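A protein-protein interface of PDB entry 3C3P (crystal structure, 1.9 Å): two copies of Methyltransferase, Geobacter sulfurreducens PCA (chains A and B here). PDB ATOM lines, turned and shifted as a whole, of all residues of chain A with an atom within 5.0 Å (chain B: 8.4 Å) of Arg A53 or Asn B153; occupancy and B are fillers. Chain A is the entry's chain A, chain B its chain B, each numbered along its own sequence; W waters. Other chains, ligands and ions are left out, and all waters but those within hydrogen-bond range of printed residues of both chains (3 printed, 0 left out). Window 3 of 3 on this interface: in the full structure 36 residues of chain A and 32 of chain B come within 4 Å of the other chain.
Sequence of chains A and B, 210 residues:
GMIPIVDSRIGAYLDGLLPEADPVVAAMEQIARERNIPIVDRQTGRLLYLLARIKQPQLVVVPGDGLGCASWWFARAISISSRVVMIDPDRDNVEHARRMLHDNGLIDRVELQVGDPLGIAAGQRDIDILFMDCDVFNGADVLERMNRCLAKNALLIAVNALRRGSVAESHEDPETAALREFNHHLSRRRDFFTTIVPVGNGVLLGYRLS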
ATOM      1  N   LEU A  48       9.031  -7.004  21.374  1.00  0.00           N
ATOM      2  CA  LEU A  48       8.167  -6.446  22.427  1.00  0.00           C
ATOM      3  C   LEU A  48       6.762  -7.004  22.288  1.00  0.00           C
ATOM      4  O   LEU A  48       6.123  -7.420  23.241  1.00  0.00           O
ATOM      5  CB  LEU A  48       8.075  -4.925  22.363  1.00  0.00           C
ATOM      6  CG  LEU A  48       9.352  -4.111  22.655  1.00  0.00           C
ATOM      7  CD1 LEU A  48       9.054  -2.592  22.693  1.00  0.00           C
ATOM      8  CD2 LEU A  48       9.984  -4.510  23.946  1.00  0.00           C
ATOM      9  N   TYR A  49       6.278  -6.945  21.068  1.00  0.00           N
ATOM     10  CA  TYR A  49       4.944  -7.490  20.745  1.00  0.00           C
ATOM     11  C   TYR A  49       4.811  -8.956  21.151  1.00  0.00           C
ATOM     12  O   TYR A  49       3.864  -9.342  21.812  1.00  0.00           O
ATOM     13  CB  TYR A  49       4.632  -7.354  19.251  1.00  0.00           C
ATOM     14  CG  TYR A  49       3.267  -7.948  18.858  1.00  0.00           C
ATOM     15  CD1 TYR A  49       2.100  -7.191  18.916  1.00  0.00           C
ATOM     16  CD2 TYR A  49       3.163  -9.277  18.461  1.00  0.00           C
ATOM     17  CE1 TYR A  49       0.857  -7.743  18.557  1.00  0.00           C
ATOM     18  CE2 TYR A  49       1.939  -9.843  18.120  1.00  0.00           C
ATOM     19  CZ  TYR A  49       0.786  -9.071  18.175  1.00  0.00           C
ATOM     20  OH  TYR A  49      -0.415  -9.656  17.825  1.00  0.00           O
ATOM     21  N   LEU A  50       5.789  -9.759  20.756  1.00  0.00           N
ATOM     22  CA  LEU A  50       5.748 -11.189  21.032  1.00  0.00           C
ATOM     23  C   LEU A  50       5.782 -11.464  22.527  1.00  0.00           C
ATOM     24  O   LEU A  50       5.010 -12.281  23.039  1.00  0.00           O
ATOM     25  CB  LEU A  50       6.832 -11.967  20.259  1.00  0.00           C
ATOM     26  CG  LEU A  50       6.668 -13.498  20.383  1.00  0.00           C
ATOM     27  CD1 LEU A  50       6.985 -14.254  19.068  1.00  0.00           C
ATOM     28  CD2 LEU A  50       7.480 -14.017  21.609  1.00  0.00           C
ATOM     29  N   LEU A  51       6.656 -10.769  23.240  1.00  0.00           N
ATOM     30  CA  LEU A  51       6.753 -10.997  24.693  1.00  0.00           C
ATOM     31  C   LEU A  51       5.439 -10.634  25.398  1.00  0.00           C
ATOM     32  O   LEU A  51       4.972 -11.297  26.344  1.00  0.00           O
ATOM     33  CB  LEU A  51       7.937 -10.189  25.280  1.00  0.00           C
ATOM     34  CG  LEU A  51       9.347 -10.643  24.887  1.00  0.00           C
ATOM     35  CD1 LEU A  51      10.379  -9.616  25.349  1.00  0.00           C
ATOM     36  CD2 LEU A  51       9.666 -12.042  25.425  1.00  0.00           C
ATOM     37  N   ALA A  52       4.813  -9.579  24.908  1.00  0.00           N
ATOM     38  CA  ALA A  52       3.573  -9.077  25.490  1.00  0.00           C
ATOM     39  C   ALA A  52       2.457 -10.061  25.211  1.00  0.00           C
ATOM     40  O   ALA A  52       1.644 -10.354  26.069  1.00  0.00           O
ATOM     41  CB  ALA A  52       3.229  -7.665  24.958  1.00  0.00           C
ATOM     42  N   ARG A  53       2.439 -10.608  24.004  1.00  0.00           N
ATOM     43  CA  ARG A  53       1.419 -11.619  23.689  1.00  0.00           C
ATOM     44  C   ARG A  53       1.541 -12.847  24.604  1.00  0.00           C
ATOM     45  O   ARG A  53       0.563 -13.356  25.107  1.00  0.00           O
ATOM     46  CB  ARG A  53       1.479 -12.100  22.247  1.00  0.00           C
ATOM     47  CG  ARG A  53       0.967 -11.142  21.199  1.00  0.00           C
ATOM     48  CD  ARG A  53      -0.469 -10.644  21.451  1.00  0.00           C
ATOM     49  NE  ARG A  53      -1.510 -11.671  21.495  1.00  0.00           N
ATOM     50  CZ  ARG A  53      -2.237 -12.073  20.455  1.00  0.00           C
ATOM     51  NH1 ARG A  53      -2.036 -11.587  19.232  1.00  0.00           N
ATOM     52  NH2 ARG A  53      -3.146 -13.005  20.657  1.00  0.00           N
ATOM     53  N   ILE A  54       2.754 -13.333  24.831  1.00  0.00           N
ATOM     54  CA  ILE A  54       2.890 -14.541  25.674  1.00  0.00           C
ATOM     55  C   ILE A  54       2.732 -14.225  27.141  1.00  0.00           C
ATOM     56  O   ILE A  54       2.300 -15.056  27.922  1.00  0.00           O
ATOM     57  CB  ILE A  54       4.194 -15.392  25.424  1.00  0.00           C
ATOM     58  CG1 ILE A  54       5.437 -14.624  25.779  1.00  0.00           C
ATOM     59  CG2 ILE A  54       4.245 -15.910  23.956  1.00  0.00           C
ATOM     60  CD1 ILE A  54       6.727 -15.504  25.783  1.00  0.00           C
ATOM     61  N   LYS A  55       3.042 -13.008  27.522  1.00  0.00           N
ATOM     62  CA  LYS A  55       2.898 -12.615  28.921  1.00  0.00           C
ATOM     63  C   LYS A  55       1.418 -12.393  29.313  1.00  0.00           C
ATOM     64  O   LYS A  55       1.013 -12.710  30.432  1.00  0.00           O
ATOM     65  CB  LYS A  55       3.634 -11.292  29.173  1.00  0.00           C
ATOM     66  CG  LYS A  55       3.634 -10.791  30.631  1.00  0.00           C
ATOM     67  CD  LYS A  55       4.601 -11.545  31.505  1.00  0.00           C
ATOM     68  CE  LYS A  55       4.674 -10.952  32.935  1.00  0.00           C
ATOM     69  NZ  LYS A  55       3.424 -11.269  33.746  1.00  0.00           N
ATOM     70  N   GLN A  56       0.645 -11.869  28.367  1.00  0.00           N
ATOM     71  CA  GLN A  56      -0.796 -11.529  28.572  1.00  0.00           C
ATOM     72  C   GLN A  56      -0.984 -10.543  29.737  1.00  0.00           C
ATOM     73  O   GLN A  56      -1.765 -10.794  30.683  1.00  0.00           O
ATOM     74  CB  GLN A  56      -1.688 -12.738  28.850  1.00  0.00           C
ATOM     75  CG  GLN A  56      -1.734 -13.806  27.808  1.00  0.00           C
ATOM     76  CD  GLN A  56      -2.967 -14.689  28.010  1.00  0.00           C
ATOM     77  OE1 GLN A  56      -3.468 -14.825  29.115  1.00  0.00           O
ATOM     78  NE2 GLN A  56      -3.473 -15.246  26.939  1.00  0.00           N
ATOM     79  N   ALA A  77      -0.795  -5.539  21.333  1.00  0.00           N
ATOM     80  CA  ALA A  77      -0.665  -6.867  21.963  1.00  0.00           C
ATOM     81  C   ALA A  77      -1.588  -7.179  23.119  1.00  0.00           C
ATOM     82  O   ALA A  77      -1.585  -8.300  23.619  1.00  0.00           O
ATOM     83  CB  ALA A  77       0.808  -7.050  22.446  1.00  0.00           C
ATOM     84  N   ILE B  54       7.274 -17.080  31.500  1.00  0.00           N
ATOM     85  CA  ILE B  54       6.348 -16.054  31.028  1.00  0.00           C
ATOM     86  C   ILE B  54       5.051 -16.649  30.455  1.00  0.00           C
ATOM     87  O   ILE B  54       3.933 -16.206  30.717  1.00  0.00           O
ATOM     88  CB  ILE B  54       7.005 -15.203  29.893  1.00  0.00           C
ATOM     89  CG1 ILE B  54       8.207 -14.379  30.400  1.00  0.00           C
ATOM     90  CG2 ILE B  54       5.995 -14.255  29.321  1.00  0.00           C
ATOM     91  CD1 ILE B  54       8.982 -13.666  29.324  1.00  0.00           C
ATOM     92  N   LYS B  55       5.258 -17.656  29.623  1.00  0.00           N
ATOM     93  CA  LYS B  55       4.150 -18.341  28.902  1.00  0.00           C
ATOM     94  C   LYS B  55       3.231 -19.152  29.818  1.00  0.00           C
ATOM     95  O   LYS B  55       2.008 -19.313  29.541  1.00  0.00           O
ATOM     96  CB  LYS B  55       4.721 -19.302  27.843  1.00  0.00           C
ATOM     97  CG  LYS B  55       3.743 -20.033  26.904  1.00  0.00           C
ATOM     98  CD  LYS B  55       3.433 -19.270  25.651  1.00  0.00           C
ATOM     99  CE  LYS B  55       2.507 -20.031  24.674  1.00  0.00           C
ATOM    100  NZ  LYS B  55       1.143 -20.296  25.221  1.00  0.00           N
ATOM    101  N   ASP B 126      -3.166 -30.010  22.159  1.00  0.00           N
ATOM    102  CA  ASP B 126      -3.118 -28.739  22.893  1.00  0.00           C
ATOM    103  C   ASP B 126      -1.748 -28.421  23.471  1.00  0.00           C
ATOM    104  O   ASP B 126      -1.586 -28.002  24.618  1.00  0.00           O
ATOM    105  CB  ASP B 126      -4.210 -28.645  23.955  1.00  0.00           C
ATOM    106  CG  ASP B 126      -5.536 -28.269  23.362  1.00  0.00           C
ATOM    107  OD1 ASP B 126      -5.549 -27.545  22.336  1.00  0.00           O
ATOM    108  OD2 ASP B 126      -6.568 -28.664  23.942  1.00  0.00           O
ATOM    109  N   ILE B 127      -0.766 -28.591  22.608  1.00  0.00           N
ATOM    110  CA  ILE B 127       0.632 -28.278  22.955  1.00  0.00           C
ATOM    111  C   ILE B 127       0.800 -26.761  23.081  1.00  0.00           C
ATOM    112  O   ILE B 127       0.467 -26.016  22.130  1.00  0.00           O
ATOM    113  CB  ILE B 127       1.610 -28.841  21.874  1.00  0.00           C
ATOM    114  CG1 ILE B 127       1.493 -30.376  21.736  1.00  0.00           C
ATOM    115  CG2 ILE B 127       3.058 -28.401  22.198  1.00  0.00           C
ATOM    116  CD1 ILE B 127       2.370 -30.977  20.608  1.00  0.00           C
ATOM    117  N   ASP B 128       1.344 -26.289  24.219  1.00  0.00           N
ATOM    118  CA  ASP B 128       1.557 -24.843  24.476  1.00  0.00           C
ATOM    119  C   ASP B 128       2.919 -24.360  23.950  1.00  0.00           C
ATOM    120  O   ASP B 128       3.072 -23.218  23.497  1.00  0.00           O
ATOM    121  CB  ASP B 128       1.386 -24.511  25.970  1.00  0.00           C
ATOM    122  CG  ASP B 128      -0.032 -24.769  26.437  1.00  0.00           C
ATOM    123  OD1 ASP B 128      -0.963 -24.275  25.768  1.00  0.00           O
ATOM    124  OD2 ASP B 128      -0.220 -25.479  27.439  1.00  0.00           O
ATOM    125  N   ILE B 129       3.919 -25.222  24.101  1.00  0.00           N
ATOM    126  CA  ILE B 129       5.262 -24.948  23.583  1.00  0.00           C
ATOM    127  C   ILE B 129       5.750 -26.168  22.875  1.00  0.00           C
ATOM    128  O   ILE B 129       5.762 -27.282  23.416  1.00  0.00           O
ATOM    129  CB  ILE B 129       6.326 -24.523  24.667  1.00  0.00           C
ATOM    130  CG1 ILE B 129       5.863 -23.269  25.393  1.00  0.00           C
ATOM    131  CG2 ILE B 129       7.746 -24.315  24.021  1.00  0.00           C
ATOM    132  CD1 ILE B 129       6.849 -22.753  26.477  1.00  0.00           C
ATOM    133  N   LEU B 150      -1.167 -28.263  18.150  1.00  0.00           N
ATOM    134  CA  LEU B 150      -0.930 -26.989  18.863  1.00  0.00           C
ATOM    135  C   LEU B 150      -2.171 -26.379  19.477  1.00  0.00           C
ATOM    136  O   LEU B 150      -3.251 -26.364  18.894  1.00  0.00           O
ATOM    137  CB  LEU B 150      -0.298 -25.940  17.945  1.00  0.00           C
ATOM    138  CG  LEU B 150       1.055 -26.290  17.338  1.00  0.00           C
ATOM    139  CD1 LEU B 150       1.439 -25.228  16.306  1.00  0.00           C
ATOM    140  CD2 LEU B 150       2.135 -26.440  18.405  1.00  0.00           C
ATOM    141  N   ALA B 151      -1.966 -25.897  20.690  1.00  0.00           N
ATOM    142  CA  ALA B 151      -2.980 -25.196  21.458  1.00  0.00           C
ATOM    143  C   ALA B 151      -3.167 -23.844  20.851  1.00  0.00           C
ATOM    144  O   ALA B 151      -2.340 -23.370  20.058  1.00  0.00           O
ATOM    145  CB  ALA B 151      -2.535 -25.000  22.920  1.00  0.00           C
ATOM    146  N   LYS B 152      -4.270 -23.213  21.228  1.00  0.00           N
ATOM    147  CA  LYS B 152      -4.501 -21.838  20.823  1.00  0.00           C
ATOM    148  C   LYS B 152      -3.312 -21.075  21.407  1.00  0.00           C
ATOM    149  O   LYS B 152      -2.926 -21.293  22.552  1.00  0.00           O
ATOM    150  CB  LYS B 152      -5.766 -21.272  21.456  1.00  0.00           C
ATOM    151  CG  LYS B 152      -6.022 -19.770  21.241  1.00  0.00           C
ATOM    152  CD  LYS B 152      -7.337 -19.299  21.905  1.00  0.00           C
ATOM    153  CE  LYS B 152      -7.592 -17.794  21.733  1.00  0.00           C
ATOM    154  N   ASN B 153      -2.773 -20.166  20.623  1.00  0.00           N
ATOM    155  CA  ASN B 153      -1.664 -19.296  21.056  1.00  0.00           C
ATOM    156  C   ASN B 153      -0.397 -20.043  21.468  1.00  0.00           C
ATOM    157  O   ASN B 153       0.397 -19.584  22.290  1.00  0.00           O
ATOM    158  CB  ASN B 153      -2.125 -18.315  22.148  1.00  0.00           C
ATOM    159  CG  ASN B 153      -3.195 -17.341  21.667  1.00  0.00           C
ATOM    160  OD1 ASN B 153      -4.040 -16.952  22.457  1.00  0.00           O
ATOM    161  ND2 ASN B 153      -3.179 -16.952  20.371  1.00  0.00           N
ATOM    162  N   ALA B 154      -0.216 -21.200  20.860  1.00  0.00           N
ATOM    163  CA  ALA B 154       0.997 -21.974  21.078  1.00  0.00           C
ATOM    164  C   ALA B 154       2.243 -21.201  20.584  1.00  0.00           C
ATOM    165  O   ALA B 154       2.183 -20.302  19.737  1.00  0.00           O
ATOM    166  CB  ALA B 154       0.921 -23.331  20.392  1.00  0.00           C
ATOM    167  N   LEU B 155       3.371 -21.539  21.193  1.00  0.00           N
ATOM    168  CA  LEU B 155       4.668 -20.971  20.815  1.00  0.00           C
ATOM    169  C   LEU B 155       5.590 -22.042  20.321  1.00  0.00           C
ATOM    170  O   LEU B 155       5.867 -23.015  21.024  1.00  0.00           O
ATOM    171  CB  LEU B 155       5.342 -20.270  22.003  1.00  0.00           C
ATOM    172  CG  LEU B 155       6.708 -19.594  21.799  1.00  0.00           C
ATOM    173  CD1 LEU B 155       6.564 -18.450  20.788  1.00  0.00           C
ATOM    174  CD2 LEU B 155       7.306 -19.120  23.168  1.00  0.00           C
ATOM    175  N   LEU B 156       6.041 -21.855  19.085  1.00  0.00           N
ATOM    176  CA  LEU B 156       7.035 -22.707  18.464  1.00  0.00           C
ATOM    177  C   LEU B 156       8.389 -22.068  18.765  1.00  0.00           C
ATOM    178  O   LEU B 156       8.592 -20.848  18.584  1.00  0.00           O
ATOM    179  CB  LEU B 156       6.880 -22.807  16.923  1.00  0.00           C
ATOM    180  CG  LEU B 156       7.917 -23.617  16.111  1.00  0.00           C
ATOM    181  CD1 LEU B 156       7.970 -25.143  16.378  1.00  0.00           C
ATOM    182  CD2 LEU B 156       7.684 -23.393  14.595  1.00  0.00           C
ATOM    183  N   ASP B 191      -1.207 -16.634  10.175  1.00  0.00           N
ATOM    184  CA  ASP B 191      -1.589 -17.350  11.396  1.00  0.00           C
ATOM    185  C   ASP B 191      -0.481 -17.438  12.457  1.00  0.00           C
ATOM    186  O   ASP B 191      -0.680 -17.978  13.530  1.00  0.00           O
ATOM    187  CB  ASP B 191      -2.190 -18.727  11.060  1.00  0.00           C
ATOM    188  CG  ASP B 191      -1.248 -19.608  10.324  1.00  0.00           C
ATOM    189  OD1 ASP B 191      -0.348 -19.073   9.643  1.00  0.00           O
ATOM    190  OD2 ASP B 191      -1.432 -20.840  10.391  1.00  0.00           O
ATOM    191  N   PHE B 192       0.675 -16.886  12.126  1.00  0.00           N
ATOM    192  CA  PHE B 192       1.820 -16.826  13.026  1.00  0.00           C
ATOM    193  C   PHE B 192       2.448 -15.479  13.060  1.00  0.00           C
ATOM    194  O   PHE B 192       2.489 -14.778  12.059  1.00  0.00           O
ATOM    195  CB  PHE B 192       2.956 -17.789  12.627  1.00  0.00           C
ATOM    196  CG  PHE B 192       2.710 -19.198  13.003  1.00  0.00           C
ATOM    197  CD1 PHE B 192       2.012 -20.046  12.160  1.00  0.00           C
ATOM    198  CD2 PHE B 192       3.170 -19.680  14.220  1.00  0.00           C
ATOM    199  CE1 PHE B 192       1.742 -21.354  12.535  1.00  0.00           C
ATOM    200  CE2 PHE B 192       2.923 -20.976  14.595  1.00  0.00           C
ATOM    201  CZ  PHE B 192       2.215 -21.823  13.752  1.00  0.00           C
ATOM    202  N   PHE B 193       2.887 -15.107  14.251  1.00  0.00           N
ATOM    203  CA  PHE B 193       3.694 -13.869  14.449  1.00  0.00           C
ATOM    204  C   PHE B 193       5.087 -14.432  14.771  1.00  0.00           C
ATOM    205  O   PHE B 193       5.303 -15.050  15.843  1.00  0.00           O
ATOM    206  CB  PHE B 193       3.190 -12.938  15.543  1.00  0.00           C
ATOM    207  CG  PHE B 193       4.026 -11.705  15.675  1.00  0.00           C
ATOM    208  CD1 PHE B 193       3.729 -10.567  14.934  1.00  0.00           C
ATOM    209  CD2 PHE B 193       5.160 -11.703  16.481  1.00  0.00           C
ATOM    210  CE1 PHE B 193       4.538  -9.438  15.064  1.00  0.00           C
ATOM    211  CE2 PHE B 193       5.962 -10.592  16.586  1.00  0.00           C
ATOM    212  CZ  PHE B 193       5.645  -9.461  15.877  1.00  0.00           C
ATOM    213  N   GLY B 206       7.867 -18.643  17.030  1.00  0.00           N
ATOM    214  CA  GLY B 206       6.656 -18.515  16.256  1.00  0.00           C
ATOM    215  C   GLY B 206       5.428 -18.650  17.131  1.00  0.00           C
ATOM    216  O   GLY B 206       5.130 -19.720  17.616  1.00  0.00           O
ATOM    217  N   TYR B 207       4.753 -17.524  17.317  1.00  0.00           N
ATOM    218  CA  TYR B 207       3.540 -17.428  18.116  1.00  0.00           C
ATOM    219  C   TYR B 207       2.294 -17.558  17.284  1.00  0.00           C
ATOM    220  O   TYR B 207       2.028 -16.776  16.377  1.00  0.00           O
ATOM    221  CB  TYR B 207       3.502 -16.091  18.859  1.00  0.00           C
ATOM    222  CG  TYR B 207       2.272 -15.845  19.701  1.00  0.00           C
ATOM    223  CD1 TYR B 207       2.156 -16.408  20.966  1.00  0.00           C
ATOM    224  CD2 TYR B 207       1.264 -14.969  19.280  1.00  0.00           C
ATOM    225  CE1 TYR B 207       1.034 -16.161  21.762  1.00  0.00           C
ATOM    226  CE2 TYR B 207       0.153 -14.722  20.073  1.00  0.00           C
ATOM    227  CZ  TYR B 207       0.058 -15.318  21.329  1.00  0.00           C
ATOM    228  OH  TYR B 207      -1.028 -15.093  22.148  1.00  0.00           O
ATOM    229  N   ARG B 208       1.508 -18.557  17.635  1.00  0.00           N
ATOM    230  CA  ARG B 208       0.238 -18.803  16.938  1.00  0.00           C
ATOM    231  C   ARG B 208      -0.821 -17.724  17.283  1.00  0.00           C
ATOM    232  O   ARG B 208      -1.226 -17.540  18.419  1.00  0.00           O
ATOM    233  CB  ARG B 208      -0.238 -20.227  17.167  1.00  0.00           C
ATOM    234  CG  ARG B 208      -1.187 -20.537  16.049  1.00  0.00           C
ATOM    235  CD  ARG B 208      -1.272 -21.974  15.682  1.00  0.00           C
ATOM    236  NE  ARG B 208      -2.020 -22.745  16.646  1.00  0.00           N
ATOM    237  CZ  ARG B 208      -3.340 -22.823  16.661  1.00  0.00           C
ATOM    238  NH1 ARG B 208      -4.048 -22.119  15.809  1.00  0.00           N
ATOM    239  NH2 ARG B 208      -3.947 -23.568  17.559  1.00  0.00           N
ATOM    240  N   LEU B 209      -1.242 -16.996  16.253  1.00  0.00           N
ATOM    241  CA  LEU B 209      -2.216 -15.882  16.386  1.00  0.00           C
ATOM    242  C   LEU B 209      -3.684 -16.293  16.535  1.00  0.00           C
ATOM    243  O   LEU B 209      -3.986 -17.469  16.465  1.00  0.00           O
ATOM    244  CB  LEU B 209      -2.093 -14.914  15.209  1.00  0.00           C
ATOM    245  CG  LEU B 209      -0.796 -14.104  15.192  1.00  0.00           C
ATOM    246  CD1 LEU B 209      -0.609 -13.408  13.840  1.00  0.00           C
ATOM    247  CD2 LEU B 209      -0.769 -13.108  16.354  1.00  0.00           C
HETATM  248  O   HOH W   1       0.754 -17.250  28.225  1.00  0.00           O
HETATM  249  O   HOH W   2      -4.070 -14.267  23.453  1.00  0.00           O
HETATM  250  O   HOH W   3       2.071 -14.723  31.769  1.00  0.00           O
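O of Ile A54 lies close to O of Ile B54 (3.4 Å).
NH2 of Arg A53 is in hydrogen-bond range of OH of Tyr B207, 3.3 Å away.
NZ of Lys B55 is in hydrogen-bond range of O of Asn B153, 3.1 Å away.
The side-chain hydroxyl of Tyr B207 sits close to the side-chain amide nitrogen of Asn B153, 3.4 Å away.
The backbone carbonyl oxygen of Asp B191 sits at hydrogen-bond distance from the backbone NH of Leu B209, at 2.9 Å.
The backbone NH (N) of Phe B193 lies within hydrogen-bond range of the backbone carbonyl oxygen (O) of Tyr B207 (2.8 Å).
The side-chain hydroxyl (OH) of Tyr A49 lies within hydrogen-bond range of the guanidinium group (NH1) of Arg A53 (2.9 Å).
O of Arg B208 is in hydrogen-bond range of ND2 of Asn B153, 2.8 Å away.
CD2 of Tyr A49 touches CZ of Phe B193 (3.6 Å).
Tyr A49 touches Leu B209.
Leu A50 touches Phe B193.
CD1 of Leu A50 touches CB of Tyr B207, at 3.9 Å.
Asn B153 touches Arg A53.
CD2 of Leu B209 touches NH1 of Arg A53, 3.5 Å away.
CG2 of Ile A54 touches CD of Lys B55 (3.8 Å).
Tyr B207 touches Ile A54 (CD1 to CG2, 3.7 Å).
Ile B54 touches Lys A55 (CG2 to CA, 3.5 Å).
Printed residues of chain B within 4 Å of Leu A50: Phe B193 (3.7 Å) and Tyr B207 (3.9 Å).
No residue of chain B comes within 4 Å of Ala A52.
Arg A53 touches three residues of chain B.
Of the printed residues of chain B, Ile A54 touches Ile B54 (3.4 Å), Lys B55 (3.8 Å) and Tyr B207 (3.7 Å).
Of the printed residues of chain A, Ile B54 touches Ile A54 (3.4 Å) and Lys A55 (3.5 Å).
Leu B150 touches none of the printed residues of chain A.
Of chain A, only Arg A53 comes within 4 Å of Asn B153.
Ala B154 touches none of the printed residues of chain A.
Of the printed residues of chain A, Tyr B207 touches Leu A50 (3.9 Å), Arg A53 (3.3 Å) and Ile A54 (3.7 Å).
The nearest residue of chain B that does not touch Arg A53 is Arg B208 (5.4 Å).
Of the 20 printed residues of chain B, 6 touch a printed residue of chain A.
Printed residues of chain B that touch a printed residue of chain A: Ile B54, Lys B55, Asn B153, Phe B193, Tyr B207 and Leu B209.
Hydrophobic or aromatic side chains of chain B that line the printed part of chain A: Ile B54, Phe B193, Tyr B207 and Leu B209.
Along chain B the printed residues that touch a printed residue of chain A span positions 54 to 209.
Of the 10 printed residues of chain A, 5 touch a printed residue of chain B.
Printed residues of chain A that touch a printed residue of chain B: Tyr A49, Leu A50, Arg A53, Ile A54 and Lys A55.
Hydrophobic or aromatic side chains of chain A that line the printed part of chain B: Tyr A49, Leu A50 and Ile A54.
Ile A54 touches its own counterpart, Ile B54.
Ile A54 touches Lys B55, and with the chains exchanged Lys A55 touches Ile B54.
2 positions are printed for both chains.
Of the 11 pairs that touch across the chains among the printed residues, 3 have their exchanged pair printed and touching as well.
Water W3 lies within hydrogen-bond range of O of Ile B54 (2.6 Å) and O of Lys A55 (2.6 Å).
Water W1 bridges the backbone carbonyl oxygen of Ile A54 (2.7 Å) and the backbone carbonyl oxygen of Lys B55 (2.7 Å).
Water W2 lies within hydrogen-bond range of the side-chain amide oxygen (OD1) of Asn B153, the guanidinium group (NH2) of Arg A53 and the side-chain hydroxyl (OH) of Tyr B207.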
